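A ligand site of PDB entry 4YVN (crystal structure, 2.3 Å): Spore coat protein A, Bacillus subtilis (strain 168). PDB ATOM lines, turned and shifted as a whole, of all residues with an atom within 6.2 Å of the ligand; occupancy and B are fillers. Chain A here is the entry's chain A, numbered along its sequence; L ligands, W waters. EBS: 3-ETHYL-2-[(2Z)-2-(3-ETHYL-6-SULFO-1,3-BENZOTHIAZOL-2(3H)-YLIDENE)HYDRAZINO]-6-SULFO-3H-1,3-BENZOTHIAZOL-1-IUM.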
ATOM      1  N   TYR A 358      18.050   7.228 -19.341  1.00  0.00           N
ATOM      2  CA  TYR A 358      17.176   7.683 -20.375  1.00  0.00           C
ATOM      3  C   TYR A 358      16.204   6.569 -20.693  1.00  0.00           C
ATOM      4  O   TYR A 358      16.493   5.383 -20.431  1.00  0.00           O
ATOM      5  CB  TYR A 358      17.971   8.070 -21.620  1.00  0.00           C
ATOM      6  CG  TYR A 358      18.729   9.362 -21.445  1.00  0.00           C
ATOM      7  CD1 TYR A 358      19.982   9.352 -20.873  1.00  0.00           C
ATOM      8  CD2 TYR A 358      18.173  10.592 -21.861  1.00  0.00           C
ATOM      9  CE1 TYR A 358      20.686  10.533 -20.729  1.00  0.00           C
ATOM     10  CE2 TYR A 358      18.863  11.793 -21.688  1.00  0.00           C
ATOM     11  CZ  TYR A 358      20.124  11.753 -21.126  1.00  0.00           C
ATOM     12  OH  TYR A 358      20.856  12.896 -20.955  1.00  0.00           O
ATOM     13  N   PRO A 359      15.026   6.936 -21.193  1.00  0.00           N
ATOM     14  CA  PRO A 359      14.204   5.872 -21.726  1.00  0.00           C
ATOM     15  C   PRO A 359      14.989   5.031 -22.752  1.00  0.00           C
ATOM     16  O   PRO A 359      15.611   5.594 -23.661  1.00  0.00           O
ATOM     17  CB  PRO A 359      13.050   6.626 -22.374  1.00  0.00           C
ATOM     18  CG  PRO A 359      12.877   7.811 -21.452  1.00  0.00           C
ATOM     19  CD  PRO A 359      14.277   8.193 -21.058  1.00  0.00           C
ATOM     20  N   SER A 360      14.975   3.703 -22.550  1.00  0.00           N
ATOM     21  CA  SER A 360      15.519   2.738 -23.503  1.00  0.00           C
ATOM     22  C   SER A 360      15.079   3.299 -24.839  1.00  0.00           C
ATOM     23  O   SER A 360      13.872   3.378 -25.144  1.00  0.00           O
ATOM     24  CB  SER A 360      15.063   1.314 -23.199  1.00  0.00           C
ATOM     25  OG  SER A 360      15.607   0.411 -24.149  1.00  0.00           O
ATOM     26  N   VAL A 361      16.077   3.683 -25.623  1.00  0.00           N
ATOM     27  CA  VAL A 361      15.932   4.151 -26.987  1.00  0.00           C
ATOM     28  C   VAL A 361      15.250   3.091 -27.887  1.00  0.00           C
ATOM     29  O   VAL A 361      14.433   3.470 -28.754  1.00  0.00           O
ATOM     30  CB  VAL A 361      17.308   4.591 -27.572  1.00  0.00           C
ATOM     31  CG1 VAL A 361      18.166   3.374 -27.976  1.00  0.00           C
ATOM     32  CG2 VAL A 361      17.133   5.581 -28.717  1.00  0.00           C
ATOM     33  N   GLN A 362      15.558   1.797 -27.688  1.00  0.00           N
ATOM     34  CA  GLN A 362      14.863   0.733 -28.426  1.00  0.00           C
ATOM     35  C   GLN A 362      13.447   0.569 -27.899  1.00  0.00           C
ATOM     36  O   GLN A 362      13.151  -0.308 -27.084  1.00  0.00           O
ATOM     37  CB  GLN A 362      15.632  -0.608 -28.456  1.00  0.00           C
ATOM     38  CG  GLN A 362      15.751  -1.401 -27.170  1.00  0.00           C
ATOM     39  CD  GLN A 362      16.511  -2.703 -27.377  1.00  0.00           C
ATOM     40  OE1 GLN A 362      16.972  -3.001 -28.482  1.00  0.00           O
ATOM     41  NE2 GLN A 362      16.649  -3.487 -26.313  1.00  0.00           N
ATOM     42  N   HIS A 363      12.580   1.474 -28.346  1.00  0.00           N
ATOM     43  CA  HIS A 363      11.156   1.318 -28.101  1.00  0.00           C
ATOM     44  C   HIS A 363      10.723   0.060 -28.808  1.00  0.00           C
ATOM     45  O   HIS A 363      11.458  -0.510 -29.625  1.00  0.00           O
ATOM     46  CB  HIS A 363      10.312   2.553 -28.533  1.00  0.00           C
ATOM     47  CG  HIS A 363      10.657   3.169 -29.868  1.00  0.00           C
ATOM     48  ND1 HIS A 363       9.886   2.988 -31.003  1.00  0.00           N
ATOM     49  CD2 HIS A 363      11.637   4.032 -30.226  1.00  0.00           C
ATOM     50  CE1 HIS A 363      10.409   3.677 -32.005  1.00  0.00           C
ATOM     51  NE2 HIS A 363      11.472   4.317 -31.554  1.00  0.00           N
ATOM     52  N   GLU A 364       9.550  -0.408 -28.450  1.00  0.00           N
ATOM     53  CA  GLU A 364       8.931  -1.486 -29.168  1.00  0.00           C
ATOM     54  C   GLU A 364       8.572  -0.962 -30.556  1.00  0.00           C
ATOM     55  O   GLU A 364       8.642   0.232 -30.823  1.00  0.00           O
ATOM     56  CB  GLU A 364       7.665  -1.925 -28.438  1.00  0.00           C
ATOM     57  CG  GLU A 364       7.520  -3.406 -28.239  1.00  0.00           C
ATOM     58  CD  GLU A 364       6.511  -3.695 -27.150  1.00  0.00           C
ATOM     59  OE1 GLU A 364       6.875  -4.364 -26.153  1.00  0.00           O
ATOM     60  OE2 GLU A 364       5.365  -3.218 -27.261  1.00  0.00           O
ATOM     61  N   ILE A 366       5.938   0.181 -33.249  1.00  0.00           N
ATOM     62  CA  ILE A 366       4.678   0.896 -33.128  1.00  0.00           C
ATOM     63  C   ILE A 366       3.581  -0.024 -33.677  1.00  0.00           C
ATOM     64  O   ILE A 366       3.502  -0.280 -34.897  1.00  0.00           O
ATOM     65  CB  ILE A 366       4.724   2.232 -33.882  1.00  0.00           C
ATOM     66  CG1 ILE A 366       5.878   3.121 -33.413  1.00  0.00           C
ATOM     67  CG2 ILE A 366       3.376   2.934 -33.797  1.00  0.00           C
ATOM     68  CD1 ILE A 366       5.966   3.388 -31.899  1.00  0.00           C
ATOM     69  N   THR A 406       2.747  -1.103 -28.058  1.00  0.00           N
ATOM     70  CA  THR A 406       3.022   0.336 -28.027  1.00  0.00           C
ATOM     71  C   THR A 406       2.258   1.014 -29.133  1.00  0.00           C
ATOM     72  O   THR A 406       2.244   0.547 -30.263  1.00  0.00           O
ATOM     73  CB  THR A 406       4.522   0.558 -28.237  1.00  0.00           C
ATOM     74  OG1 THR A 406       5.249  -0.183 -27.269  1.00  0.00           O
ATOM     75  CG2 THR A 406       4.885   1.994 -28.099  1.00  0.00           C
ATOM     76  N   GLU A 407       1.613   2.126 -28.812  1.00  0.00           N
ATOM     77  CA  GLU A 407       0.912   2.941 -29.747  1.00  0.00           C
ATOM     78  C   GLU A 407       1.398   4.376 -29.680  1.00  0.00           C
ATOM     79  O   GLU A 407       1.899   4.812 -28.667  1.00  0.00           O
ATOM     80  CB  GLU A 407      -0.595   2.935 -29.444  1.00  0.00           C
ATOM     81  CG  GLU A 407      -1.197   1.547 -29.282  1.00  0.00           C
ATOM     82  CD  GLU A 407      -2.703   1.573 -29.319  1.00  0.00           C
ATOM     83  OE1 GLU A 407      -3.317   2.635 -28.951  1.00  0.00           O
ATOM     84  OE2 GLU A 407      -3.274   0.529 -29.720  1.00  0.00           O
ATOM     85  N   ILE A 408       1.247   5.084 -30.782  1.00  0.00           N
ATOM     86  CA  ILE A 408       1.329   6.517 -30.815  1.00  0.00           C
ATOM     87  C   ILE A 408      -0.098   7.041 -30.865  1.00  0.00           C
ATOM     88  O   ILE A 408      -0.919   6.517 -31.638  1.00  0.00           O
ATOM     89  CB  ILE A 408       2.070   7.014 -32.059  1.00  0.00           C
ATOM     90  CG1 ILE A 408       3.535   6.641 -31.937  1.00  0.00           C
ATOM     91  CG2 ILE A 408       1.919   8.510 -32.162  1.00  0.00           C
ATOM     92  CD1 ILE A 408       4.361   6.953 -33.189  1.00  0.00           C
ATOM     93  N   SER A 427       2.343   5.456 -18.167  1.00  0.00           N
ATOM     94  CA  SER A 427       2.939   6.724 -18.546  1.00  0.00           C
ATOM     95  C   SER A 427       3.375   6.635 -19.978  1.00  0.00           C
ATOM     96  O   SER A 427       3.445   5.531 -20.540  1.00  0.00           O
ATOM     97  CB  SER A 427       4.078   7.185 -17.627  1.00  0.00           C
ATOM     98  OG  SER A 427       4.674   6.182 -16.896  1.00  0.00           O
ATOM     99  N   PHE A 428       3.664   7.794 -20.541  1.00  0.00           N
ATOM    100  CA  PHE A 428       3.989   7.981 -21.926  1.00  0.00           C
ATOM    101  C   PHE A 428       5.094   9.026 -22.157  1.00  0.00           C
ATOM    102  O   PHE A 428       5.445   9.811 -21.259  1.00  0.00           O
ATOM    103  CB  PHE A 428       2.726   8.378 -22.717  1.00  0.00           C
ATOM    104  CG  PHE A 428       1.935   9.518 -22.144  1.00  0.00           C
ATOM    105  CD1 PHE A 428       2.306  10.838 -22.394  1.00  0.00           C
ATOM    106  CD2 PHE A 428       0.737   9.286 -21.457  1.00  0.00           C
ATOM    107  CE1 PHE A 428       1.545  11.904 -21.941  1.00  0.00           C
ATOM    108  CE2 PHE A 428      -0.005  10.335 -20.968  1.00  0.00           C
ATOM    109  CZ  PHE A 428       0.392  11.649 -21.202  1.00  0.00           C
ATOM    110  N   ARG A 429       5.674   8.964 -23.362  1.00  0.00           N
ATOM    111  CA  ARG A 429       6.699   9.884 -23.850  1.00  0.00           C
ATOM    112  C   ARG A 429       5.962  10.893 -24.639  1.00  0.00           C
ATOM    113  O   ARG A 429       4.934  10.587 -25.239  1.00  0.00           O
ATOM    114  CB  ARG A 429       7.639   9.186 -24.815  1.00  0.00           C
ATOM    115  CG  ARG A 429       8.386   8.033 -24.238  1.00  0.00           C
ATOM    116  CD  ARG A 429       9.248   8.430 -23.066  1.00  0.00           C
ATOM    117  NE  ARG A 429      10.252   9.470 -23.398  1.00  0.00           N
ATOM    118  CZ  ARG A 429      11.346   9.298 -24.156  1.00  0.00           C
ATOM    119  NH1 ARG A 429      12.170  10.323 -24.372  1.00  0.00           N
ATOM    120  NH2 ARG A 429      11.604   8.126 -24.722  1.00  0.00           N
ATOM    121  N   VAL A 430       6.465  12.097 -24.632  1.00  0.00           N
ATOM    122  CA  VAL A 430       5.918  13.173 -25.459  1.00  0.00           C
ATOM    123  C   VAL A 430       6.805  13.262 -26.696  1.00  0.00           C
ATOM    124  O   VAL A 430       8.027  13.403 -26.581  1.00  0.00           O
ATOM    125  CB  VAL A 430       5.888  14.497 -24.708  1.00  0.00           C
ATOM    126  CG1 VAL A 430       5.225  15.570 -25.536  1.00  0.00           C
ATOM    127  CG2 VAL A 430       5.110  14.327 -23.425  1.00  0.00           C
ATOM    128  N   LEU A 431       6.210  13.119 -27.874  1.00  0.00           N
ATOM    129  CA  LEU A 431       7.013  13.004 -29.083  1.00  0.00           C
ATOM    130  C   LEU A 431       7.232  14.399 -29.661  1.00  0.00           C
ATOM    131  O   LEU A 431       8.380  14.823 -29.832  1.00  0.00           O
ATOM    132  CB  LEU A 431       6.349  12.074 -30.085  1.00  0.00           C
ATOM    133  CG  LEU A 431       6.177  10.603 -29.736  1.00  0.00           C
ATOM    134  CD1 LEU A 431       5.757   9.843 -30.994  1.00  0.00           C
ATOM    135  CD2 LEU A 431       7.465  10.029 -29.156  1.00  0.00           C
ATOM    136  N   ASP A 432       6.129  15.134 -29.881  1.00  0.00           N
ATOM    137  CA  ASP A 432       6.208  16.496 -30.427  1.00  0.00           C
ATOM    138  C   ASP A 432       4.843  17.164 -30.494  1.00  0.00           C
ATOM    139  O   ASP A 432       3.843  16.520 -30.275  1.00  0.00           O
ATOM    140  CB  ASP A 432       6.818  16.470 -31.840  1.00  0.00           C
ATOM    141  CG  ASP A 432       6.208  15.405 -32.700  1.00  0.00           C
ATOM    142  OD1 ASP A 432       4.932  15.300 -32.785  1.00  0.00           O
ATOM    143  OD2 ASP A 432       7.003  14.638 -33.241  1.00  0.00           O
ATOM    144  N   TRP A 463       8.826  10.910 -18.433  1.00  0.00           N
ATOM    145  CA  TRP A 463       7.591  10.186 -18.490  1.00  0.00           C
ATOM    146  C   TRP A 463       6.498  11.045 -17.911  1.00  0.00           C
ATOM    147  O   TRP A 463       6.628  11.600 -16.806  1.00  0.00           O
ATOM    148  CB  TRP A 463       7.705   8.914 -17.699  1.00  0.00           C
ATOM    149  CG  TRP A 463       8.627   7.899 -18.292  1.00  0.00           C
ATOM    150  CD1 TRP A 463       9.881   7.577 -17.852  1.00  0.00           C
ATOM    151  CD2 TRP A 463       8.371   7.062 -19.427  1.00  0.00           C
ATOM    152  NE1 TRP A 463      10.416   6.577 -18.634  1.00  0.00           N
ATOM    153  CE2 TRP A 463       9.507   6.250 -19.618  1.00  0.00           C
ATOM    154  CE3 TRP A 463       7.286   6.913 -20.303  1.00  0.00           C
ATOM    155  CZ2 TRP A 463       9.596   5.288 -20.633  1.00  0.00           C
ATOM    156  CZ3 TRP A 463       7.354   5.954 -21.314  1.00  0.00           C
ATOM    157  CH2 TRP A 463       8.516   5.156 -21.477  1.00  0.00           C
ATOM    158  N   ARG A 476       1.622  14.597 -30.056  1.00  0.00           N
ATOM    159  CA  ARG A 476       1.831  13.159 -30.214  1.00  0.00           C
ATOM    160  C   ARG A 476       2.531  12.581 -28.995  1.00  0.00           C
ATOM    161  O   ARG A 476       3.534  13.118 -28.545  1.00  0.00           O
ATOM    162  CB  ARG A 476       2.642  12.815 -31.485  1.00  0.00           C
ATOM    163  CG  ARG A 476       1.983  13.263 -32.783  1.00  0.00           C
ATOM    164  CD  ARG A 476       2.580  12.532 -34.020  1.00  0.00           C
ATOM    165  NE  ARG A 476       4.023  12.700 -34.010  1.00  0.00           N
ATOM    166  CZ  ARG A 476       4.912  11.772 -34.296  1.00  0.00           C
ATOM    167  NH1 ARG A 476       6.202  12.043 -34.156  1.00  0.00           N
ATOM    168  NH2 ARG A 476       4.513  10.593 -34.720  1.00  0.00           N
ATOM    169  N   ALA A 478       3.524   8.581 -26.994  1.00  0.00           N
ATOM    170  CA  ALA A 478       3.721   7.151 -27.217  1.00  0.00           C
ATOM    171  C   ALA A 478       3.666   6.433 -25.901  1.00  0.00           C
ATOM    172  O   ALA A 478       4.302   6.863 -24.924  1.00  0.00           O
ATOM    173  CB  ALA A 478       5.079   6.891 -27.887  1.00  0.00           C
ATOM    174  N   ALA A 479       2.924   5.321 -25.855  1.00  0.00           N
ATOM    175  CA  ALA A 479       2.784   4.550 -24.607  1.00  0.00           C
ATOM    176  C   ALA A 479       2.830   3.077 -24.884  1.00  0.00           C
ATOM    177  O   ALA A 479       2.333   2.651 -25.906  1.00  0.00           O
ATOM    178  CB  ALA A 479       1.466   4.885 -23.922  1.00  0.00           C
ATOM    179  N   THR A 480       3.375   2.317 -23.957  1.00  0.00           N
ATOM    180  CA  THR A 480       3.279   0.882 -23.991  1.00  0.00           C
ATOM    181  C   THR A 480       2.204   0.461 -23.021  1.00  0.00           C
ATOM    182  O   THR A 480       2.257   0.797 -21.846  1.00  0.00           O
ATOM    183  CB  THR A 480       4.617   0.199 -23.631  1.00  0.00           C
ATOM    184  OG1 THR A 480       5.603   0.602 -24.595  1.00  0.00           O
ATOM    185  CG2 THR A 480       4.454  -1.355 -23.690  1.00  0.00           C
HETATM  186  C1  EBS L   1      10.406   3.605 -24.222  1.00  0.00           C
HETATM  187  C2  EBS L   1       9.057   3.005 -24.439  1.00  0.00           C
HETATM  188  C3  EBS L   1      11.205   3.169 -23.166  1.00  0.00           C
HETATM  189  C4  EBS L   1       8.627   1.989 -23.564  1.00  0.00           C
HETATM  190  C5  EBS L   1      10.740   2.152 -22.322  1.00  0.00           C
HETATM  191  C6  EBS L   1       9.461   1.560 -22.519  1.00  0.00           C
HETATM  192  N7  EBS L   1       8.500   3.608 -25.503  1.00  0.00           N
HETATM  193  C8  EBS L   1       9.316   4.561 -26.015  1.00  0.00           C
HETATM  194  S9  EBS L   1      10.883   4.816 -25.302  1.00  0.00           S
HETATM  195  C10 EBS L   1       8.797   7.309 -31.040  1.00  0.00           C
HETATM  196  C11 EBS L   1       9.991   8.128 -30.646  1.00  0.00           C
HETATM  197  C12 EBS L   1       8.228   7.477 -32.308  1.00  0.00           C
HETATM  198  C13 EBS L   1      10.502   9.055 -31.566  1.00  0.00           C
HETATM  199  C14 EBS L   1       8.768   8.437 -33.197  1.00  0.00           C
HETATM  200  C15 EBS L   1       9.887   9.218 -32.826  1.00  0.00           C
HETATM  201  N16 EBS L   1      10.354   7.799 -29.381  1.00  0.00           N
HETATM  202  C17 EBS L   1       9.522   6.821 -28.906  1.00  0.00           C
HETATM  203  S18 EBS L   1       8.227   6.197 -29.898  1.00  0.00           S
HETATM  204  N19 EBS L   1       9.738   6.292 -27.651  1.00  0.00           N
HETATM  205  N20 EBS L   1       8.924   5.294 -27.099  1.00  0.00           N
HETATM  206  C21 EBS L   1      11.507   8.400 -28.658  1.00  0.00           C
HETATM  207  C22 EBS L   1      11.158   9.729 -28.005  1.00  0.00           C
HETATM  208  S23 EBS L   1       8.133   8.644 -34.668  1.00  0.00           S
HETATM  209  C24 EBS L   1       7.192   3.275 -26.015  1.00  0.00           C
HETATM  210  C25 EBS L   1       6.205   4.185 -25.289  1.00  0.00           C
HETATM  211  S26 EBS L   1      11.661   1.699 -21.067  1.00  0.00           S
HETATM  212  O39 EBS L   1       6.713   8.396 -34.738  1.00  0.00           O
HETATM  213  O45 EBS L   1      12.672   2.692 -20.818  1.00  0.00           O
HETATM  214  O46 EBS L   1      12.221   0.170 -21.144  1.00  0.00           O
HETATM  215  O47 EBS L   1      10.770   1.663 -19.942  1.00  0.00           O
HETATM  216  O48 EBS L   1       8.968   7.637 -35.637  1.00  0.00           O
HETATM  217  O49 EBS L   1       8.295  10.011 -35.087  1.00  0.00           O
HETATM  218  O   HOH W   1      13.136   4.711 -18.055  1.00  0.00           O
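A sulfur (S18) of the ligand lies close to a ring nitrogen (ND1) of His 363 (3.8 Å).
The backbone NH (N) of Ser 360 is in hydrogen-bond range of an oxygen (O45) of the ligand.
The guanidinium group (NH1) of Arg 476 lies within salt-bridge range of an oxygen (O49) of the ligand, at 3.1 Å.
NH2 of Arg 429 sits close to S9 of the ligand (3.4 Å).
Water W1 lies within hydrogen-bond range of the indole nitrogen of Trp 463 and an oxygen (O45) of the ligand.
The backbone NH of Ala 479 sits at hydrogen-bond distance from the backbone carbonyl oxygen of Glu 407 (3.0 Å).
N of Arg 429 sits at hydrogen-bond distance from O of Ala 478 (3.0 Å).
The side-chain hydroxyl (OG1) of Thr 406 sits at hydrogen-bond distance from the side-chain carboxylate (OE2) of Glu 364 (3.0 Å).
The backbone NH (N) of Leu 431 lies within hydrogen-bond range of the backbone carbonyl oxygen (O) of Arg 476.
The guanidinium group (NH1) of Arg 476 lies within salt-bridge range of the side-chain carboxylate (OD2) of Asp 432 (2.9 Å).
The side-chain hydroxyl (OG1) of Thr 406 sits at hydrogen-bond distance from the side-chain hydroxyl (OG1) of Thr 480 (2.8 Å).
Residues that only touch the ligand: Pro 359, Thr 406, Ile 408, Leu 431, Trp 463, Ala 478, Ala 479 and Thr 480.
Hydrophobic or aromatic side chains that line the ligand: Pro 359, His 363, Ile 408, Leu 431, Trp 463 and Ala 478.
12 residues have an atom within 4 Å of the ligand: Pro 359, Ser 360, His 363, Thr 406, Ile 408, Arg 429, Leu 431, Trp 463, Arg 476, Ala 478, Ala 479 and Thr 480.
The nearest printed residue that does not touch the ligand is Ile 366 (4.1 Å).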
